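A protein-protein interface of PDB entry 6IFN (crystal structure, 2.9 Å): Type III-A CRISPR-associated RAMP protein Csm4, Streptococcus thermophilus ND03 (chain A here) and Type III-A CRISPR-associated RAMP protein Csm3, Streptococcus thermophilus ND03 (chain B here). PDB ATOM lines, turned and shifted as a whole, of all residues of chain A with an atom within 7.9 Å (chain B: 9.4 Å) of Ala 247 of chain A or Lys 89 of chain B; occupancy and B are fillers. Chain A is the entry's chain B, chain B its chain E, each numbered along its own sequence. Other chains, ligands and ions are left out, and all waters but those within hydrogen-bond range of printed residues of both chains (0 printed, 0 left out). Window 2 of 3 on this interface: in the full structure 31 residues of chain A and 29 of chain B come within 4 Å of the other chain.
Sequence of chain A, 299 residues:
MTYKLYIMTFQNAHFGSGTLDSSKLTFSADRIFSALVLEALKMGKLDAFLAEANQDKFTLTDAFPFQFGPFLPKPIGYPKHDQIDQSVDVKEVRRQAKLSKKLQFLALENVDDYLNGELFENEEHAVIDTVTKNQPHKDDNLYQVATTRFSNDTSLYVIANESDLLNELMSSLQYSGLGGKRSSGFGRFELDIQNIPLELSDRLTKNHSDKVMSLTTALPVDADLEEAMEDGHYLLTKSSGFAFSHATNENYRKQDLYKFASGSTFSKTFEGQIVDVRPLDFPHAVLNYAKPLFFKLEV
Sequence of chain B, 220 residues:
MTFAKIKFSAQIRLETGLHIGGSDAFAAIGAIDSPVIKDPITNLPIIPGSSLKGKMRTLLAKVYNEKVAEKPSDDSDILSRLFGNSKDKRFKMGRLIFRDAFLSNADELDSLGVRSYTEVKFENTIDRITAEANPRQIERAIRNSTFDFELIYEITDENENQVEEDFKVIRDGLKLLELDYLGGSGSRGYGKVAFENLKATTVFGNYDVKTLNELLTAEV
The backbone NH (N) of Lys 89 of chain B is in hydrogen-bond range of the side-chain amide oxygen (OD1) of Asn 249 of chain A (2.5 Å). The side-chain amino group (NZ) of Lys 92 of chain B is in hydrogen-bond range of the backbone carbonyl oxygen (O) of Thr 248 of chain A. The side-chain amino group (NZ) of Lys 92 of chain B is in hydrogen-bond range of the backbone carbonyl oxygen (O) of Asn 249 of chain A (2.8 Å). NZ of Lys 92 of chain B lies within hydrogen-bond range of O of Glu 250 of chain A (3.5 Å).
The side-chain amide oxygen of Asn 85 of chain B sits at hydrogen-bond distance from the backbone NH of Lys 87 of chain B (2.9 Å). OD1 of Asn 85 of chain B is in hydrogen-bond range of N of Asp 88 of chain B (3.4 Å). The side-chain carboxylate (OD2) of Asp 88 of chain B lies within salt-bridge range of the guanidinium group (NH2) of Arg 90 of chain B, 2.7 Å away. The side-chain hydroxyl of Ser 245 of chain A sits at hydrogen-bond distance from the backbone NH of Ala 247 of chain A, at 3.1 Å. OG of Ser 245 of chain A sits close to NE2 of His 284 of chain A (3.5 Å). The backbone carbonyl oxygen (O) of Glu 250 of chain A sits at hydrogen-bond distance from the side-chain hydroxyl (OG1) of Thr 248 of chain A (3.1 Å).
Met 93 of chain B touches Phe 244 of chain A (CG to CZ, 3.5 Å). Ser 245 of chain A touches Lys 92 of chain B. Lys 89 of chain B touches His 246 of chain A. O of Arg 90 of chain B touches CD2 of His 246 of chain A (3.7 Å). Lys 89 of chain B touches Ala 247 of chain A. C of Thr 248 of chain A touches CB of Lys 89 of chain B, at 3.8 Å. CG of Asn 249 of chain A touches O of Lys 87 of chain B, 3.6 Å away. C of Asp 88 of chain B touches OD1 of Asn 249 of chain A, at 3.4 Å.
Of chain B, only Lys 89 comes within 4 Å of Ala 247 of chain A. Thr 248 of chain A touches just these residues of chain B: Lys 89 (3.8 Å) and Lys 92 (3.1 Å). Printed residues of chain B within 4 Å of Phe 244 of chain A: Met 93 (3.5 Å). Printed residues of chain B within 4 Å of Glu 250 of chain A: Lys 92 (3.5 Å). Of the printed residues of chain A, Lys 87 of chain B touches Asn 249 (3.6 Å). Printed residues of chain B within 4 Å of Asn 249 of chain A: Lys 87, Asp 88, Lys 89 and Lys 92. Of the printed residues of chain A, Met 93 of chain B touches Phe 244. Phe 282 of chain A touches none of the printed residues of chain B. Ser 80 of chain B touches none of the printed residues of chain A. The nearest residue of chain B that does not touch Ala 247 of chain A is Lys 92 of chain B (6.7 Å). The nearest printed residue of chain B that does not touch Phe 244 of chain A is Lys 92 of chain B (4.02 Å).
Printed residues of chain B that touch a printed residue of chain A: Lys 87, Asp 88, Lys 89, Arg 90, Lys 92 and Met 93. Hydrophobic or aromatic side chains of chain B within 4 Å of the printed part of chain A: Met 93. Along chain B the printed residues that touch a printed residue of chain A span positions 87 to 93. Of the 11 printed residues of chain A, 7 touch a printed residue of chain B. Printed residues of chain A that touch a printed residue of chain B: Phe 244, Ser 245, His 246, Ala 247, Thr 248, Asn 249 and Glu 250. Among the printed residues, 12 pairs touch across the chains.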
ATOM      1  N   ALA A 243     -27.627  10.284   4.739  1.00  0.00           N
ATOM      2  CA  ALA A 243     -28.858  10.121   4.011  1.00  0.00           C
ATOM      3  C   ALA A 243     -28.754  10.897   2.707  1.00  0.00           C
ATOM      4  O   ALA A 243     -28.495  12.065   2.715  1.00  0.00           O
ATOM      5  CB  ALA A 243     -30.005  10.621   4.843  1.00  0.00           C
ATOM      6  N   PHE A 244     -28.981  10.235   1.586  1.00  0.00           N
ATOM      7  CA  PHE A 244     -28.989  10.947   0.332  1.00  0.00           C
ATOM      8  C   PHE A 244     -30.342  11.643   0.150  1.00  0.00           C
ATOM      9  O   PHE A 244     -31.387  11.030   0.395  1.00  0.00           O
ATOM     10  CB  PHE A 244     -28.716   9.983  -0.816  1.00  0.00           C
ATOM     11  CG  PHE A 244     -28.609  10.696  -2.130  1.00  0.00           C
ATOM     12  CD1 PHE A 244     -27.543  11.531  -2.390  1.00  0.00           C
ATOM     13  CD2 PHE A 244     -29.614  10.594  -3.062  1.00  0.00           C
ATOM     14  CE1 PHE A 244     -27.464  12.222  -3.584  1.00  0.00           C
ATOM     15  CE2 PHE A 244     -29.536  11.278  -4.257  1.00  0.00           C
ATOM     16  CZ  PHE A 244     -28.452  12.080  -4.522  1.00  0.00           C
ATOM     17  N   SER A 245     -30.331  12.916  -0.270  1.00  0.00           N
ATOM     18  CA  SER A 245     -31.592  13.683  -0.393  1.00  0.00           C
ATOM     19  C   SER A 245     -31.352  15.089  -0.945  1.00  0.00           C
ATOM     20  O   SER A 245     -30.289  15.674  -0.753  1.00  0.00           O
ATOM     21  CB  SER A 245     -32.324  13.800   0.925  1.00  0.00           C
ATOM     22  OG  SER A 245     -32.116  15.086   1.481  1.00  0.00           O
ATOM     23  N   HIS A 246     -32.412  15.633  -1.548  1.00  0.00           N
ATOM     24  CA  HIS A 246     -32.397  16.933  -2.133  1.00  0.00           C
ATOM     25  C   HIS A 246     -33.040  17.928  -1.175  1.00  0.00           C
ATOM     26  O   HIS A 246     -33.165  19.090  -1.476  1.00  0.00           O
ATOM     27  CB  HIS A 246     -33.132  16.889  -3.470  1.00  0.00           C
ATOM     28  CG  HIS A 246     -32.520  15.965  -4.472  1.00  0.00           C
ATOM     29  ND1 HIS A 246     -33.030  14.695  -4.721  1.00  0.00           N
ATOM     30  CD2 HIS A 246     -31.448  16.127  -5.291  1.00  0.00           C
ATOM     31  CE1 HIS A 246     -32.304  14.128  -5.668  1.00  0.00           C
ATOM     32  NE2 HIS A 246     -31.317  14.989  -6.034  1.00  0.00           N
ATOM     33  N   ALA A 247     -33.465  17.432  -0.023  1.00  0.00           N
ATOM     34  CA  ALA A 247     -34.140  18.217   0.974  1.00  0.00           C
ATOM     35  C   ALA A 247     -33.270  19.388   1.404  1.00  0.00           C
ATOM     36  O   ALA A 247     -33.754  20.472   1.505  1.00  0.00           O
ATOM     37  CB  ALA A 247     -34.464  17.362   2.174  1.00  0.00           C
ATOM     38  N   THR A 248     -31.997  19.122   1.689  1.00  0.00           N
ATOM     39  CA  THR A 248     -31.137  20.076   2.361  1.00  0.00           C
ATOM     40  C   THR A 248     -29.732  20.026   1.786  1.00  0.00           C
ATOM     41  O   THR A 248     -29.292  19.004   1.368  1.00  0.00           O
ATOM     42  CB  THR A 248     -31.017  19.721   3.838  1.00  0.00           C
ATOM     43  OG1 THR A 248     -30.411  18.430   3.869  1.00  0.00           O
ATOM     44  CG2 THR A 248     -32.353  19.677   4.537  1.00  0.00           C
ATOM     45  N   ASN A 249     -29.020  21.142   1.856  1.00  0.00           N
ATOM     46  CA  ASN A 249     -27.633  21.179   1.423  1.00  0.00           C
ATOM     47  C   ASN A 249     -26.755  20.380   2.387  1.00  0.00           C
ATOM     48  O   ASN A 249     -25.845  19.672   1.941  1.00  0.00           O
ATOM     49  CB  ASN A 249     -27.140  22.615   1.277  1.00  0.00           C
ATOM     50  CG  ASN A 249     -27.981  23.397   0.293  1.00  0.00           C
ATOM     51  OD1 ASN A 249     -28.507  22.818  -0.651  1.00  0.00           O
ATOM     52  ND2 ASN A 249     -28.141  24.692   0.517  1.00  0.00           N
ATOM     53  N   GLU A 250     -27.031  20.472   3.692  1.00  0.00           N
ATOM     54  CA  GLU A 250     -26.157  19.832   4.685  1.00  0.00           C
ATOM     55  C   GLU A 250     -26.328  18.308   4.596  1.00  0.00           C
ATOM     56  O   GLU A 250     -27.366  17.834   4.091  1.00  0.00           O
ATOM     57  CB  GLU A 250     -26.458  20.324   6.100  1.00  0.00           C
ATOM     58  CG  GLU A 250     -26.387  21.826   6.269  1.00  0.00           C
ATOM     59  CD  GLU A 250     -27.508  22.564   5.556  1.00  0.00           C
ATOM     60  OE1 GLU A 250     -28.705  22.252   5.827  1.00  0.00           O
ATOM     61  OE2 GLU A 250     -27.180  23.424   4.695  1.00  0.00           O
ATOM     62  N   PHE A 282     -36.031  15.461  10.471  1.00  0.00           N
ATOM     63  CA  PHE A 282     -35.667  15.643   9.077  1.00  0.00           C
ATOM     64  C   PHE A 282     -36.929  15.796   8.237  1.00  0.00           C
ATOM     65  O   PHE A 282     -37.909  15.089   8.463  1.00  0.00           O
ATOM     66  CB  PHE A 282     -34.855  14.431   8.591  1.00  0.00           C
ATOM     67  CG  PHE A 282     -33.912  14.638   7.426  1.00  0.00           C
ATOM     68  CD1 PHE A 282     -32.706  15.300   7.594  1.00  0.00           C
ATOM     69  CD2 PHE A 282     -34.188  14.071   6.194  1.00  0.00           C
ATOM     70  CE1 PHE A 282     -31.838  15.463   6.532  1.00  0.00           C
ATOM     71  CE2 PHE A 282     -33.305  14.211   5.136  1.00  0.00           C
ATOM     72  CZ  PHE A 282     -32.137  14.915   5.305  1.00  0.00           C
ATOM     73  N   PRO A 283     -36.928  16.687   7.220  1.00  0.00           N
ATOM     74  CA  PRO A 283     -38.041  16.836   6.280  1.00  0.00           C
ATOM     75  C   PRO A 283     -38.725  15.558   5.791  1.00  0.00           C
ATOM     76  O   PRO A 283     -39.881  15.564   5.656  1.00  0.00           O
ATOM     77  CB  PRO A 283     -37.431  17.471   5.019  1.00  0.00           C
ATOM     78  CG  PRO A 283     -35.958  17.702   5.377  1.00  0.00           C
ATOM     79  CD  PRO A 283     -35.844  17.611   6.889  1.00  0.00           C
ATOM     80  N   HIS A 284     -37.996  14.506   5.457  1.00  0.00           N
ATOM     81  CA  HIS A 284     -38.652  13.351   4.880  1.00  0.00           C
ATOM     82  C   HIS A 284     -38.134  12.069   5.513  1.00  0.00           C
ATOM     83  O   HIS A 284     -37.055  12.059   6.078  1.00  0.00           O
ATOM     84  CB  HIS A 284     -38.494  13.331   3.352  1.00  0.00           C
ATOM     85  CG  HIS A 284     -37.103  13.154   2.853  1.00  0.00           C
ATOM     86  ND1 HIS A 284     -36.493  11.924   2.811  1.00  0.00           N
ATOM     87  CD2 HIS A 284     -36.232  14.051   2.330  1.00  0.00           C
ATOM     88  CE1 HIS A 284     -35.273  12.076   2.318  1.00  0.00           C
ATOM     89  NE2 HIS A 284     -35.084  13.379   2.006  1.00  0.00           N
ATOM     90  N   SER B  80     -23.304  22.388 -12.800  1.00  0.00           N
ATOM     91  CA  SER B  80     -23.681  21.655 -11.590  1.00  0.00           C
ATOM     92  C   SER B  80     -24.852  20.727 -11.912  1.00  0.00           C
ATOM     93  O   SER B  80     -24.881  19.606 -11.444  1.00  0.00           O
ATOM     94  CB  SER B  80     -24.011  22.593 -10.452  1.00  0.00           C
ATOM     95  OG  SER B  80     -22.847  23.287 -10.012  1.00  0.00           O
ATOM     96  N   GLY B  84     -23.054  17.497 -11.193  1.00  0.00           N
ATOM     97  CA  GLY B  84     -23.378  17.361  -9.784  1.00  0.00           C
ATOM     98  C   GLY B  84     -22.582  18.333  -8.927  1.00  0.00           C
ATOM     99  O   GLY B  84     -21.484  18.747  -9.278  1.00  0.00           O
ATOM    100  N   ASN B  85     -23.205  18.722  -7.814  1.00  0.00           N
ATOM    101  CA  ASN B  85     -22.689  19.671  -6.866  1.00  0.00           C
ATOM    102  C   ASN B  85     -23.061  19.156  -5.475  1.00  0.00           C
ATOM    103  O   ASN B  85     -24.220  18.983  -5.170  1.00  0.00           O
ATOM    104  CB  ASN B  85     -23.264  21.056  -7.124  1.00  0.00           C
ATOM    105  CG  ASN B  85     -22.682  22.106  -6.206  1.00  0.00           C
ATOM    106  OD1 ASN B  85     -22.338  21.819  -5.066  1.00  0.00           O
ATOM    107  ND2 ASN B  85     -22.569  23.327  -6.698  1.00  0.00           N
ATOM    108  N   SER B  86     -22.059  18.884  -4.643  1.00  0.00           N
ATOM    109  CA  SER B  86     -22.289  18.211  -3.364  1.00  0.00           C
ATOM    110  C   SER B  86     -22.885  19.183  -2.337  1.00  0.00           C
ATOM    111  O   SER B  86     -23.477  18.726  -1.362  1.00  0.00           O
ATOM    112  CB  SER B  86     -21.043  17.576  -2.829  1.00  0.00           C
ATOM    113  OG  SER B  86     -19.919  18.416  -3.027  1.00  0.00           O
ATOM    114  N   LYS B  87     -22.735  20.498  -2.559  1.00  0.00           N
ATOM    115  CA  LYS B  87     -23.144  21.531  -1.583  1.00  0.00           C
ATOM    116  C   LYS B  87     -24.460  22.213  -2.008  1.00  0.00           C
ATOM    117  O   LYS B  87     -24.856  23.173  -1.395  1.00  0.00           O
ATOM    118  CB  LYS B  87     -22.018  22.536  -1.395  1.00  0.00           C
ATOM    119  N   ASP B  88     -25.132  21.719  -3.049  1.00  0.00           N
ATOM    120  CA  ASP B  88     -26.370  22.324  -3.543  1.00  0.00           C
ATOM    121  C   ASP B  88     -27.473  21.258  -3.546  1.00  0.00           C
ATOM    122  O   ASP B  88     -27.388  20.270  -4.244  1.00  0.00           O
ATOM    123  CB  ASP B  88     -26.174  22.924  -4.940  1.00  0.00           C
ATOM    124  CG  ASP B  88     -27.298  23.801  -5.455  1.00  0.00           C
ATOM    125  OD1 ASP B  88     -28.445  23.471  -5.149  1.00  0.00           O
ATOM    126  OD2 ASP B  88     -27.001  24.787  -6.196  1.00  0.00           O
ATOM    127  N   LYS B  89     -28.538  21.502  -2.783  1.00  0.00           N
ATOM    128  CA  LYS B  89     -29.615  20.546  -2.591  1.00  0.00           C
ATOM    129  C   LYS B  89     -30.221  20.121  -3.935  1.00  0.00           C
ATOM    130  O   LYS B  89     -30.662  18.990  -4.051  1.00  0.00           O
ATOM    131  CB  LYS B  89     -30.697  21.127  -1.679  1.00  0.00           C
ATOM    132  CG  LYS B  89     -31.412  22.355  -2.226  1.00  0.00           C
ATOM    133  CD  LYS B  89     -32.735  22.694  -1.504  1.00  0.00           C
ATOM    134  CE  LYS B  89     -32.592  23.183  -0.077  1.00  0.00           C
ATOM    135  NZ  LYS B  89     -31.482  24.152   0.102  1.00  0.00           N
ATOM    136  N   ARG B  90     -30.232  21.004  -4.939  1.00  0.00           N
ATOM    137  CA  ARG B  90     -30.923  20.733  -6.197  1.00  0.00           C
ATOM    138  C   ARG B  90     -30.130  19.731  -7.040  1.00  0.00           C
ATOM    139  O   ARG B  90     -30.716  18.889  -7.712  1.00  0.00           O
ATOM    140  CB  ARG B  90     -31.111  22.016  -7.008  1.00  0.00           C
ATOM    141  CG  ARG B  90     -31.921  23.104  -6.318  1.00  0.00           C
ATOM    142  CD  ARG B  90     -31.804  24.449  -7.027  1.00  0.00           C
ATOM    143  NE  ARG B  90     -30.502  25.067  -6.821  1.00  0.00           N
ATOM    144  CZ  ARG B  90     -30.020  26.082  -7.526  1.00  0.00           C
ATOM    145  NH1 ARG B  90     -30.804  26.731  -8.360  1.00  0.00           N
ATOM    146  NH2 ARG B  90     -28.754  26.439  -7.418  1.00  0.00           N
ATOM    147  N   PHE B  91     -28.797  19.847  -7.010  1.00  0.00           N
ATOM    148  CA  PHE B  91     -27.948  19.159  -7.961  1.00  0.00           C
ATOM    149  C   PHE B  91     -27.073  18.097  -7.301  1.00  0.00           C
ATOM    150  O   PHE B  91     -26.103  17.681  -7.908  1.00  0.00           O
ATOM    151  CB  PHE B  91     -27.001  20.135  -8.643  1.00  0.00           C
ATOM    152  CG  PHE B  91     -27.685  21.356  -9.165  1.00  0.00           C
ATOM    153  CD1 PHE B  91     -28.663  21.241 -10.139  1.00  0.00           C
ATOM    154  CD2 PHE B  91     -27.370  22.596  -8.653  1.00  0.00           C
ATOM    155  CE1 PHE B  91     -29.338  22.357 -10.593  1.00  0.00           C
ATOM    156  CE2 PHE B  91     -28.015  23.716  -9.136  1.00  0.00           C
ATOM    157  CZ  PHE B  91     -29.002  23.592 -10.099  1.00  0.00           C
ATOM    158  N   LYS B  92     -27.439  17.603  -6.119  1.00  0.00           N
ATOM    159  CA  LYS B  92     -26.534  16.728  -5.382  1.00  0.00           C
ATOM    160  C   LYS B  92     -25.998  15.604  -6.264  1.00  0.00           C
ATOM    161  O   LYS B  92     -24.884  15.185  -6.067  1.00  0.00           O
ATOM    162  CB  LYS B  92     -27.179  16.199  -4.106  1.00  0.00           C
ATOM    163  CG  LYS B  92     -27.015  17.163  -2.937  1.00  0.00           C
ATOM    164  CD  LYS B  92     -26.669  16.514  -1.616  1.00  0.00           C
ATOM    165  CE  LYS B  92     -26.176  17.535  -0.613  1.00  0.00           C
ATOM    166  NZ  LYS B  92     -26.778  17.328   0.724  1.00  0.00           N
ATOM    167  N   MET B  93     -26.779  15.160  -7.246  1.00  0.00           N
ATOM    168  CA  MET B  93     -26.264  14.325  -8.345  1.00  0.00           C
ATOM    169  C   MET B  93     -26.612  14.986  -9.680  1.00  0.00           C
ATOM    170  O   MET B  93     -27.754  15.321  -9.946  1.00  0.00           O
ATOM    171  CB  MET B  93     -26.890  12.938  -8.293  1.00  0.00           C
ATOM    172  CG  MET B  93     -26.242  12.044  -7.280  1.00  0.00           C
ATOM    173  SD  MET B  93     -26.350  10.361  -7.892  1.00  0.00           S
ATOM    174  CE  MET B  93     -24.976  10.412  -9.037  1.00  0.00           C
ATOM    175  N   GLY B  94     -25.633  15.096 -10.570  1.00  0.00           N
ATOM    176  CA  GLY B  94     -25.865  15.591 -11.917  1.00  0.00           C
ATOM    177  C   GLY B  94     -26.749  14.663 -12.740  1.00  0.00           C
ATOM    178  O   GLY B  94     -27.173  13.624 -12.282  1.00  0.00           O
